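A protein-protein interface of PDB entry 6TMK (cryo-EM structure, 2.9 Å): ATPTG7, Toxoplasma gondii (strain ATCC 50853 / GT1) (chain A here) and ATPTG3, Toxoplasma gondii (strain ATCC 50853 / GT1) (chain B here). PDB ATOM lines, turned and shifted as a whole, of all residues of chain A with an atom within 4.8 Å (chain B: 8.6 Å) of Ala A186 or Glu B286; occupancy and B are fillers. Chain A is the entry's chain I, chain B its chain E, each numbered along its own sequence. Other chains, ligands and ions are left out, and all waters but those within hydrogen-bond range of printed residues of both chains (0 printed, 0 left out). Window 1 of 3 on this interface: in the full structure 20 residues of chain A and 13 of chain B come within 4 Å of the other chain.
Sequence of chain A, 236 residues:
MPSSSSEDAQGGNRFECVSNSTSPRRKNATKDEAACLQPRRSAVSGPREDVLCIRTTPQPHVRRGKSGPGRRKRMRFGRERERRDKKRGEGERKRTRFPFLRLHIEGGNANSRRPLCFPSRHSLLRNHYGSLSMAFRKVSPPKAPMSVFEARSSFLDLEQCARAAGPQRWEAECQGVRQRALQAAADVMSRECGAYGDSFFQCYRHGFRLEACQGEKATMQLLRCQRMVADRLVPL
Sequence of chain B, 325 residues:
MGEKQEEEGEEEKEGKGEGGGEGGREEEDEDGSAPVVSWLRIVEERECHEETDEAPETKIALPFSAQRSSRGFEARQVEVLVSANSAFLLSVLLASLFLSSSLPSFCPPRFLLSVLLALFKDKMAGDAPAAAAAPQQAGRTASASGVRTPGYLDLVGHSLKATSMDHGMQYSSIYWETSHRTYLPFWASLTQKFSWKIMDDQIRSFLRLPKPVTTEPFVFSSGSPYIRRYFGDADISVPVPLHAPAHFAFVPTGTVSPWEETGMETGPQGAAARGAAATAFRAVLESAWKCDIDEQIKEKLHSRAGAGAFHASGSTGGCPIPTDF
Of the printed residues of chain B, Leu A182 touches Lys B290 (3.9 Å) and Ile B293 (3.9 Å).
Ala A185 touches just one residue of chain B: Trp B289.
Printed residues of chain B within 4 Å of Ala A186: Glu B286 and Trp B289.
Glu B286 touches just these residues of chain A: Gln A183 (3.0 Å), Ala A186 (3.3 Å) and Ser A190 (3.2 Å).
Of the printed residues of chain A, Lys B290 touches Leu A182 and Gln A183.
The side-chain carboxylate (OE2) of Glu B286 lies within salt-bridge range of the side-chain amino group (NZ) of Lys B290 (3.8 Å).
The side-chain hydroxyl (OG) of Ser A190 is in hydrogen-bond range of the backbone carbonyl oxygen (O) of Ala A186.
The side-chain amide nitrogen (NE2) of Gln A183 lies within hydrogen-bond range of the side-chain carboxylate (OE2) of Glu B286 (3.0 Å).
The side-chain hydroxyl (OG) of Ser A190 is in hydrogen-bond range of the side-chain carboxylate (OE1) of Glu B286, 3.2 Å away.
CD of Lys B290 touches O of Leu A182, at 3.9 Å.
CG2 of Ile B293 touches CD2 of Leu A182 (3.9 Å).
Gln A183 touches Lys B290.
Ala A185 touches Trp B289.
Ala A186 touches Glu B286 (CB to CG, 3.3 Å).
N of Ala A186 touches CZ3 of Trp B289, at 3.7 Å.
Met A189 touches Trp B289 (CG to CE2, 3.9 Å).
Ser A190 touches Arg B282.
Of the 9 printed residues of chain A, 6 touch a printed residue of chain B.
Printed residues of chain A that touch a printed residue of chain B: Leu A182, Gln A183, Ala A185, Ala A186, Met A189 and Ser A190.
Along chain A the printed residues that touch a printed residue of chain B span positions 182 to 190.
Of the 15 printed residues of chain B, 5 touch a printed residue of chain A.
Hydrophobic or aromatic side chains of chain B within 4 Å of the printed part of chain A: Trp B289 and Ile B293.
Along chain B the printed residues that touch a printed residue of chain A span positions 282 to 293.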
ATOM      1  N   LEU A 182     -27.149   1.077   8.822  1.00  0.00           N
ATOM      2  CA  LEU A 182     -27.720   2.416   8.754  1.00  0.00           C
ATOM      3  C   LEU A 182     -26.677   3.480   9.061  1.00  0.00           C
ATOM      4  O   LEU A 182     -26.666   4.541   8.429  1.00  0.00           O
ATOM      5  CB  LEU A 182     -28.897   2.534   9.714  1.00  0.00           C
ATOM      6  CG  LEU A 182     -30.143   1.723   9.371  1.00  0.00           C
ATOM      7  CD1 LEU A 182     -31.192   1.951  10.424  1.00  0.00           C
ATOM      8  CD2 LEU A 182     -30.684   2.091   8.010  1.00  0.00           C
ATOM      9  N   GLN A 183     -25.768   3.207   9.996  1.00  0.00           N
ATOM     10  CA  GLN A 183     -24.746   4.192  10.328  1.00  0.00           C
ATOM     11  C   GLN A 183     -23.763   4.369   9.181  1.00  0.00           C
ATOM     12  O   GLN A 183     -23.334   5.493   8.889  1.00  0.00           O
ATOM     13  CB  GLN A 183     -24.016   3.769  11.600  1.00  0.00           C
ATOM     14  CG  GLN A 183     -23.120   4.833  12.196  1.00  0.00           C
ATOM     15  CD  GLN A 183     -23.881   6.067  12.628  1.00  0.00           C
ATOM     16  OE1 GLN A 183     -24.506   6.083  13.689  1.00  0.00           O
ATOM     17  NE2 GLN A 183     -23.836   7.109  11.808  1.00  0.00           N
ATOM     18  N   ALA A 184     -23.405   3.278   8.505  1.00  0.00           N
ATOM     19  CA  ALA A 184     -22.502   3.388   7.366  1.00  0.00           C
ATOM     20  C   ALA A 184     -23.159   4.141   6.215  1.00  0.00           C
ATOM     21  O   ALA A 184     -22.544   5.025   5.600  1.00  0.00           O
ATOM     22  CB  ALA A 184     -22.061   1.998   6.922  1.00  0.00           C
ATOM     23  N   ALA A 185     -24.411   3.800   5.905  1.00  0.00           N
ATOM     24  CA  ALA A 185     -25.140   4.533   4.877  1.00  0.00           C
ATOM     25  C   ALA A 185     -25.266   6.006   5.237  1.00  0.00           C
ATOM     26  O   ALA A 185     -25.208   6.875   4.362  1.00  0.00           O
ATOM     27  CB  ALA A 185     -26.516   3.910   4.676  1.00  0.00           C
ATOM     28  N   ALA A 186     -25.424   6.305   6.524  1.00  0.00           N
ATOM     29  CA  ALA A 186     -25.537   7.688   6.964  1.00  0.00           C
ATOM     30  C   ALA A 186     -24.225   8.436   6.790  1.00  0.00           C
ATOM     31  O   ALA A 186     -24.216   9.609   6.402  1.00  0.00           O
ATOM     32  CB  ALA A 186     -25.982   7.723   8.417  1.00  0.00           C
ATOM     33  N   ASP A 187     -23.107   7.779   7.090  1.00  0.00           N
ATOM     34  CA  ASP A 187     -21.803   8.377   6.833  1.00  0.00           C
ATOM     35  C   ASP A 187     -21.643   8.695   5.352  1.00  0.00           C
ATOM     36  O   ASP A 187     -21.193   9.786   4.980  1.00  0.00           O
ATOM     37  CB  ASP A 187     -20.700   7.438   7.307  1.00  0.00           C
ATOM     38  CG  ASP A 187     -20.802   7.116   8.783  1.00  0.00           C
ATOM     39  OD1 ASP A 187     -20.517   5.962   9.162  1.00  0.00           O
ATOM     40  OD2 ASP A 187     -21.173   8.016   9.563  1.00  0.00           O
ATOM     41  N   VAL A 188     -22.000   7.740   4.493  1.00  0.00           N
ATOM     42  CA  VAL A 188     -21.911   7.970   3.054  1.00  0.00           C
ATOM     43  C   VAL A 188     -22.776   9.156   2.650  1.00  0.00           C
ATOM     44  O   VAL A 188     -22.354  10.013   1.862  1.00  0.00           O
ATOM     45  CB  VAL A 188     -22.315   6.698   2.291  1.00  0.00           C
ATOM     46  CG1 VAL A 188     -22.451   6.989   0.823  1.00  0.00           C
ATOM     47  CG2 VAL A 188     -21.308   5.614   2.522  1.00  0.00           C
ATOM     48  N   MET A 189     -24.002   9.214   3.167  1.00  0.00           N
ATOM     49  CA  MET A 189     -24.910  10.298   2.814  1.00  0.00           C
ATOM     50  C   MET A 189     -24.348  11.639   3.247  1.00  0.00           C
ATOM     51  O   MET A 189     -24.412  12.616   2.499  1.00  0.00           O
ATOM     52  CB  MET A 189     -26.278  10.069   3.448  1.00  0.00           C
ATOM     53  CG  MET A 189     -27.393  10.888   2.832  1.00  0.00           C
ATOM     54  SD  MET A 189     -27.406  12.611   3.356  1.00  0.00           S
ATOM     55  CE  MET A 189     -27.795  12.443   5.092  1.00  0.00           C
ATOM     56  N   SER A 190     -23.823  11.714   4.467  1.00  0.00           N
ATOM     57  CA  SER A 190     -23.287  12.975   4.957  1.00  0.00           C
ATOM     58  C   SER A 190     -22.089  13.411   4.129  1.00  0.00           C
ATOM     59  O   SER A 190     -21.934  14.599   3.824  1.00  0.00           O
ATOM     60  CB  SER A 190     -22.902  12.839   6.426  1.00  0.00           C
ATOM     61  OG  SER A 190     -24.047  12.892   7.257  1.00  0.00           O
ATOM     62  N   THR B 279     -23.068  21.080  12.187  1.00  0.00           N
ATOM     63  CA  THR B 279     -22.900  19.672  12.517  1.00  0.00           C
ATOM     64  C   THR B 279     -24.183  19.091  13.093  1.00  0.00           C
ATOM     65  O   THR B 279     -24.564  17.959  12.772  1.00  0.00           O
ATOM     66  CB  THR B 279     -21.740  19.506  13.500  1.00  0.00           C
ATOM     67  OG1 THR B 279     -20.591  20.202  13.010  1.00  0.00           O
ATOM     68  CG2 THR B 279     -21.394  18.045  13.691  1.00  0.00           C
ATOM     69  N   ALA B 280     -24.869  19.856  13.942  1.00  0.00           N
ATOM     70  CA  ALA B 280     -26.137  19.403  14.491  1.00  0.00           C
ATOM     71  C   ALA B 280     -27.192  19.254  13.403  1.00  0.00           C
ATOM     72  O   ALA B 280     -27.959  18.284  13.397  1.00  0.00           O
ATOM     73  CB  ALA B 280     -26.607  20.385  15.556  1.00  0.00           C
ATOM     74  N   PHE B 281     -27.254  20.214  12.481  1.00  0.00           N
ATOM     75  CA  PHE B 281     -28.173  20.110  11.354  1.00  0.00           C
ATOM     76  C   PHE B 281     -27.888  18.863  10.531  1.00  0.00           C
ATOM     77  O   PHE B 281     -28.811  18.149  10.116  1.00  0.00           O
ATOM     78  CB  PHE B 281     -28.065  21.372  10.506  1.00  0.00           C
ATOM     79  CG  PHE B 281     -28.992  21.401   9.337  1.00  0.00           C
ATOM     80  CD1 PHE B 281     -30.350  21.532   9.521  1.00  0.00           C
ATOM     81  CD2 PHE B 281     -28.504  21.330   8.052  1.00  0.00           C
ATOM     82  CE1 PHE B 281     -31.198  21.565   8.454  1.00  0.00           C
ATOM     83  CE2 PHE B 281     -29.351  21.365   6.981  1.00  0.00           C
ATOM     84  CZ  PHE B 281     -30.700  21.487   7.181  1.00  0.00           C
ATOM     85  N   ARG B 282     -26.610  18.596  10.278  1.00  0.00           N
ATOM     86  CA  ARG B 282     -26.219  17.404   9.540  1.00  0.00           C
ATOM     87  C   ARG B 282     -26.650  16.141  10.271  1.00  0.00           C
ATOM     88  O   ARG B 282     -27.133  15.189   9.651  1.00  0.00           O
ATOM     89  CB  ARG B 282     -24.710  17.421   9.327  1.00  0.00           C
ATOM     90  CG  ARG B 282     -24.209  16.480   8.277  1.00  0.00           C
ATOM     91  CD  ARG B 282     -22.733  16.677   8.075  1.00  0.00           C
ATOM     92  NE  ARG B 282     -22.460  17.905   7.338  1.00  0.00           N
ATOM     93  CZ  ARG B 282     -21.381  18.102   6.591  1.00  0.00           C
ATOM     94  NH1 ARG B 282     -20.461  17.159   6.481  1.00  0.00           N
ATOM     95  NH2 ARG B 282     -21.222  19.250   5.955  1.00  0.00           N
ATOM     96  N   ALA B 283     -26.502  16.125  11.595  1.00  0.00           N
ATOM     97  CA  ALA B 283     -26.927  14.972  12.379  1.00  0.00           C
ATOM     98  C   ALA B 283     -28.439  14.783  12.324  1.00  0.00           C
ATOM     99  O   ALA B 283     -28.930  13.650  12.292  1.00  0.00           O
ATOM    100  CB  ALA B 283     -26.467  15.138  13.818  1.00  0.00           C
ATOM    101  N   VAL B 284     -29.191  15.880  12.322  1.00  0.00           N
ATOM    102  CA  VAL B 284     -30.644  15.784  12.257  1.00  0.00           C
ATOM    103  C   VAL B 284     -31.078  15.219  10.912  1.00  0.00           C
ATOM    104  O   VAL B 284     -31.955  14.346  10.832  1.00  0.00           O
ATOM    105  CB  VAL B 284     -31.275  17.162  12.517  1.00  0.00           C
ATOM    106  CG1 VAL B 284     -32.749  17.133  12.212  1.00  0.00           C
ATOM    107  CG2 VAL B 284     -31.040  17.578  13.935  1.00  0.00           C
ATOM    108  N   LEU B 285     -30.488  15.729   9.830  1.00  0.00           N
ATOM    109  CA  LEU B 285     -30.759  15.169   8.514  1.00  0.00           C
ATOM    110  C   LEU B 285     -30.406  13.693   8.474  1.00  0.00           C
ATOM    111  O   LEU B 285     -31.127  12.882   7.881  1.00  0.00           O
ATOM    112  CB  LEU B 285     -29.971  15.922   7.450  1.00  0.00           C
ATOM    113  CG  LEU B 285     -30.250  17.407   7.260  1.00  0.00           C
ATOM    114  CD1 LEU B 285     -29.580  17.854   5.996  1.00  0.00           C
ATOM    115  CD2 LEU B 285     -31.719  17.718   7.210  1.00  0.00           C
ATOM    116  N   GLU B 286     -29.288  13.334   9.097  1.00  0.00           N
ATOM    117  CA  GLU B 286     -28.865  11.946   9.172  1.00  0.00           C
ATOM    118  C   GLU B 286     -29.924  11.083   9.844  1.00  0.00           C
ATOM    119  O   GLU B 286     -30.269  10.002   9.352  1.00  0.00           O
ATOM    120  CB  GLU B 286     -27.544  11.884   9.927  1.00  0.00           C
ATOM    121  CG  GLU B 286     -26.823  10.592   9.834  1.00  0.00           C
ATOM    122  CD  GLU B 286     -25.433  10.665  10.428  1.00  0.00           C
ATOM    123  OE1 GLU B 286     -24.708  11.635  10.119  1.00  0.00           O
ATOM    124  OE2 GLU B 286     -25.066   9.759  11.205  1.00  0.00           O
ATOM    125  N   SER B 287     -30.465  11.560  10.962  1.00  0.00           N
ATOM    126  CA  SER B 287     -31.468  10.796  11.693  1.00  0.00           C
ATOM    127  C   SER B 287     -32.741  10.627  10.874  1.00  0.00           C
ATOM    128  O   SER B 287     -33.316   9.532  10.815  1.00  0.00           O
ATOM    129  CB  SER B 287     -31.771  11.487  13.017  1.00  0.00           C
ATOM    130  OG  SER B 287     -32.972  11.004  13.578  1.00  0.00           O
ATOM    131  N   ALA B 288     -33.207  11.704  10.246  1.00  0.00           N
ATOM    132  CA  ALA B 288     -34.422  11.611   9.443  1.00  0.00           C
ATOM    133  C   ALA B 288     -34.236  10.662   8.261  1.00  0.00           C
ATOM    134  O   ALA B 288     -35.116   9.839   7.959  1.00  0.00           O
ATOM    135  CB  ALA B 288     -34.821  13.000   8.963  1.00  0.00           C
ATOM    136  N   TRP B 289     -33.092  10.760   7.585  1.00  0.00           N
ATOM    137  CA  TRP B 289     -32.781   9.841   6.499  1.00  0.00           C
ATOM    138  C   TRP B 289     -32.757   8.402   6.990  1.00  0.00           C
ATOM    139  O   TRP B 289     -33.225   7.493   6.294  1.00  0.00           O
ATOM    140  CB  TRP B 289     -31.442  10.231   5.884  1.00  0.00           C
ATOM    141  CG  TRP B 289     -31.150   9.578   4.589  1.00  0.00           C
ATOM    142  CD1 TRP B 289     -31.720   9.856   3.390  1.00  0.00           C
ATOM    143  CD2 TRP B 289     -30.202   8.538   4.353  1.00  0.00           C
ATOM    144  NE1 TRP B 289     -31.190   9.051   2.417  1.00  0.00           N
ATOM    145  CE2 TRP B 289     -30.253   8.231   2.985  1.00  0.00           C
ATOM    146  CE3 TRP B 289     -29.314   7.836   5.167  1.00  0.00           C
ATOM    147  CZ2 TRP B 289     -29.455   7.254   2.413  1.00  0.00           C
ATOM    148  CZ3 TRP B 289     -28.525   6.866   4.597  1.00  0.00           C
ATOM    149  CH2 TRP B 289     -28.599   6.583   3.235  1.00  0.00           C
ATOM    150  N   LYS B 290     -32.210   8.172   8.181  1.00  0.00           N
ATOM    151  CA  LYS B 290     -32.163   6.822   8.724  1.00  0.00           C
ATOM    152  C   LYS B 290     -33.563   6.295   8.995  1.00  0.00           C
ATOM    153  O   LYS B 290     -33.848   5.118   8.758  1.00  0.00           O
ATOM    154  CB  LYS B 290     -31.321   6.794   9.993  1.00  0.00           C
ATOM    155  CG  LYS B 290     -29.862   6.554   9.733  1.00  0.00           C
ATOM    156  CD  LYS B 290     -29.103   6.280  11.002  1.00  0.00           C
ATOM    157  CE  LYS B 290     -28.797   7.541  11.748  1.00  0.00           C
ATOM    158  NZ  LYS B 290     -27.663   7.341  12.671  1.00  0.00           N
ATOM    159  N   CYS B 291     -34.452   7.156   9.483  1.00  0.00           N
ATOM    160  CA  CYS B 291     -35.842   6.749   9.677  1.00  0.00           C
ATOM    161  C   CYS B 291     -36.467   6.307   8.360  1.00  0.00           C
ATOM    162  O   CYS B 291     -37.080   5.230   8.266  1.00  0.00           O
ATOM    163  CB  CYS B 291     -36.639   7.904  10.281  1.00  0.00           C
ATOM    164  SG  CYS B 291     -36.387   8.173  12.047  1.00  0.00           S
ATOM    165  N   ASP B 292     -36.312   7.128   7.321  1.00  0.00           N
ATOM    166  CA  ASP B 292     -36.898   6.797   6.025  1.00  0.00           C
ATOM    167  C   ASP B 292     -36.332   5.487   5.481  1.00  0.00           C
ATOM    168  O   ASP B 292     -37.075   4.628   4.984  1.00  0.00           O
ATOM    169  CB  ASP B 292     -36.659   7.936   5.041  1.00  0.00           C
ATOM    170  CG  ASP B 292     -37.374   9.209   5.436  1.00  0.00           C
ATOM    171  OD1 ASP B 292     -38.443   9.117   6.075  1.00  0.00           O
ATOM    172  OD2 ASP B 292     -36.873  10.302   5.103  1.00  0.00           O
ATOM    173  N   ILE B 293     -35.012   5.316   5.562  1.00  0.00           N
ATOM    174  CA  ILE B 293     -34.395   4.115   5.016  1.00  0.00           C
ATOM    175  C   ILE B 293     -34.759   2.887   5.834  1.00  0.00           C
ATOM    176  O   ILE B 293     -34.849   1.781   5.291  1.00  0.00           O
ATOM    177  CB  ILE B 293     -32.872   4.298   4.943  1.00  0.00           C
ATOM    178  CG1 ILE B 293     -32.520   5.427   3.979  1.00  0.00           C
ATOM    179  CG2 ILE B 293     -32.207   3.016   4.516  1.00  0.00           C
ATOM    180  CD1 ILE B 293     -32.952   5.194   2.564  1.00  0.00           C
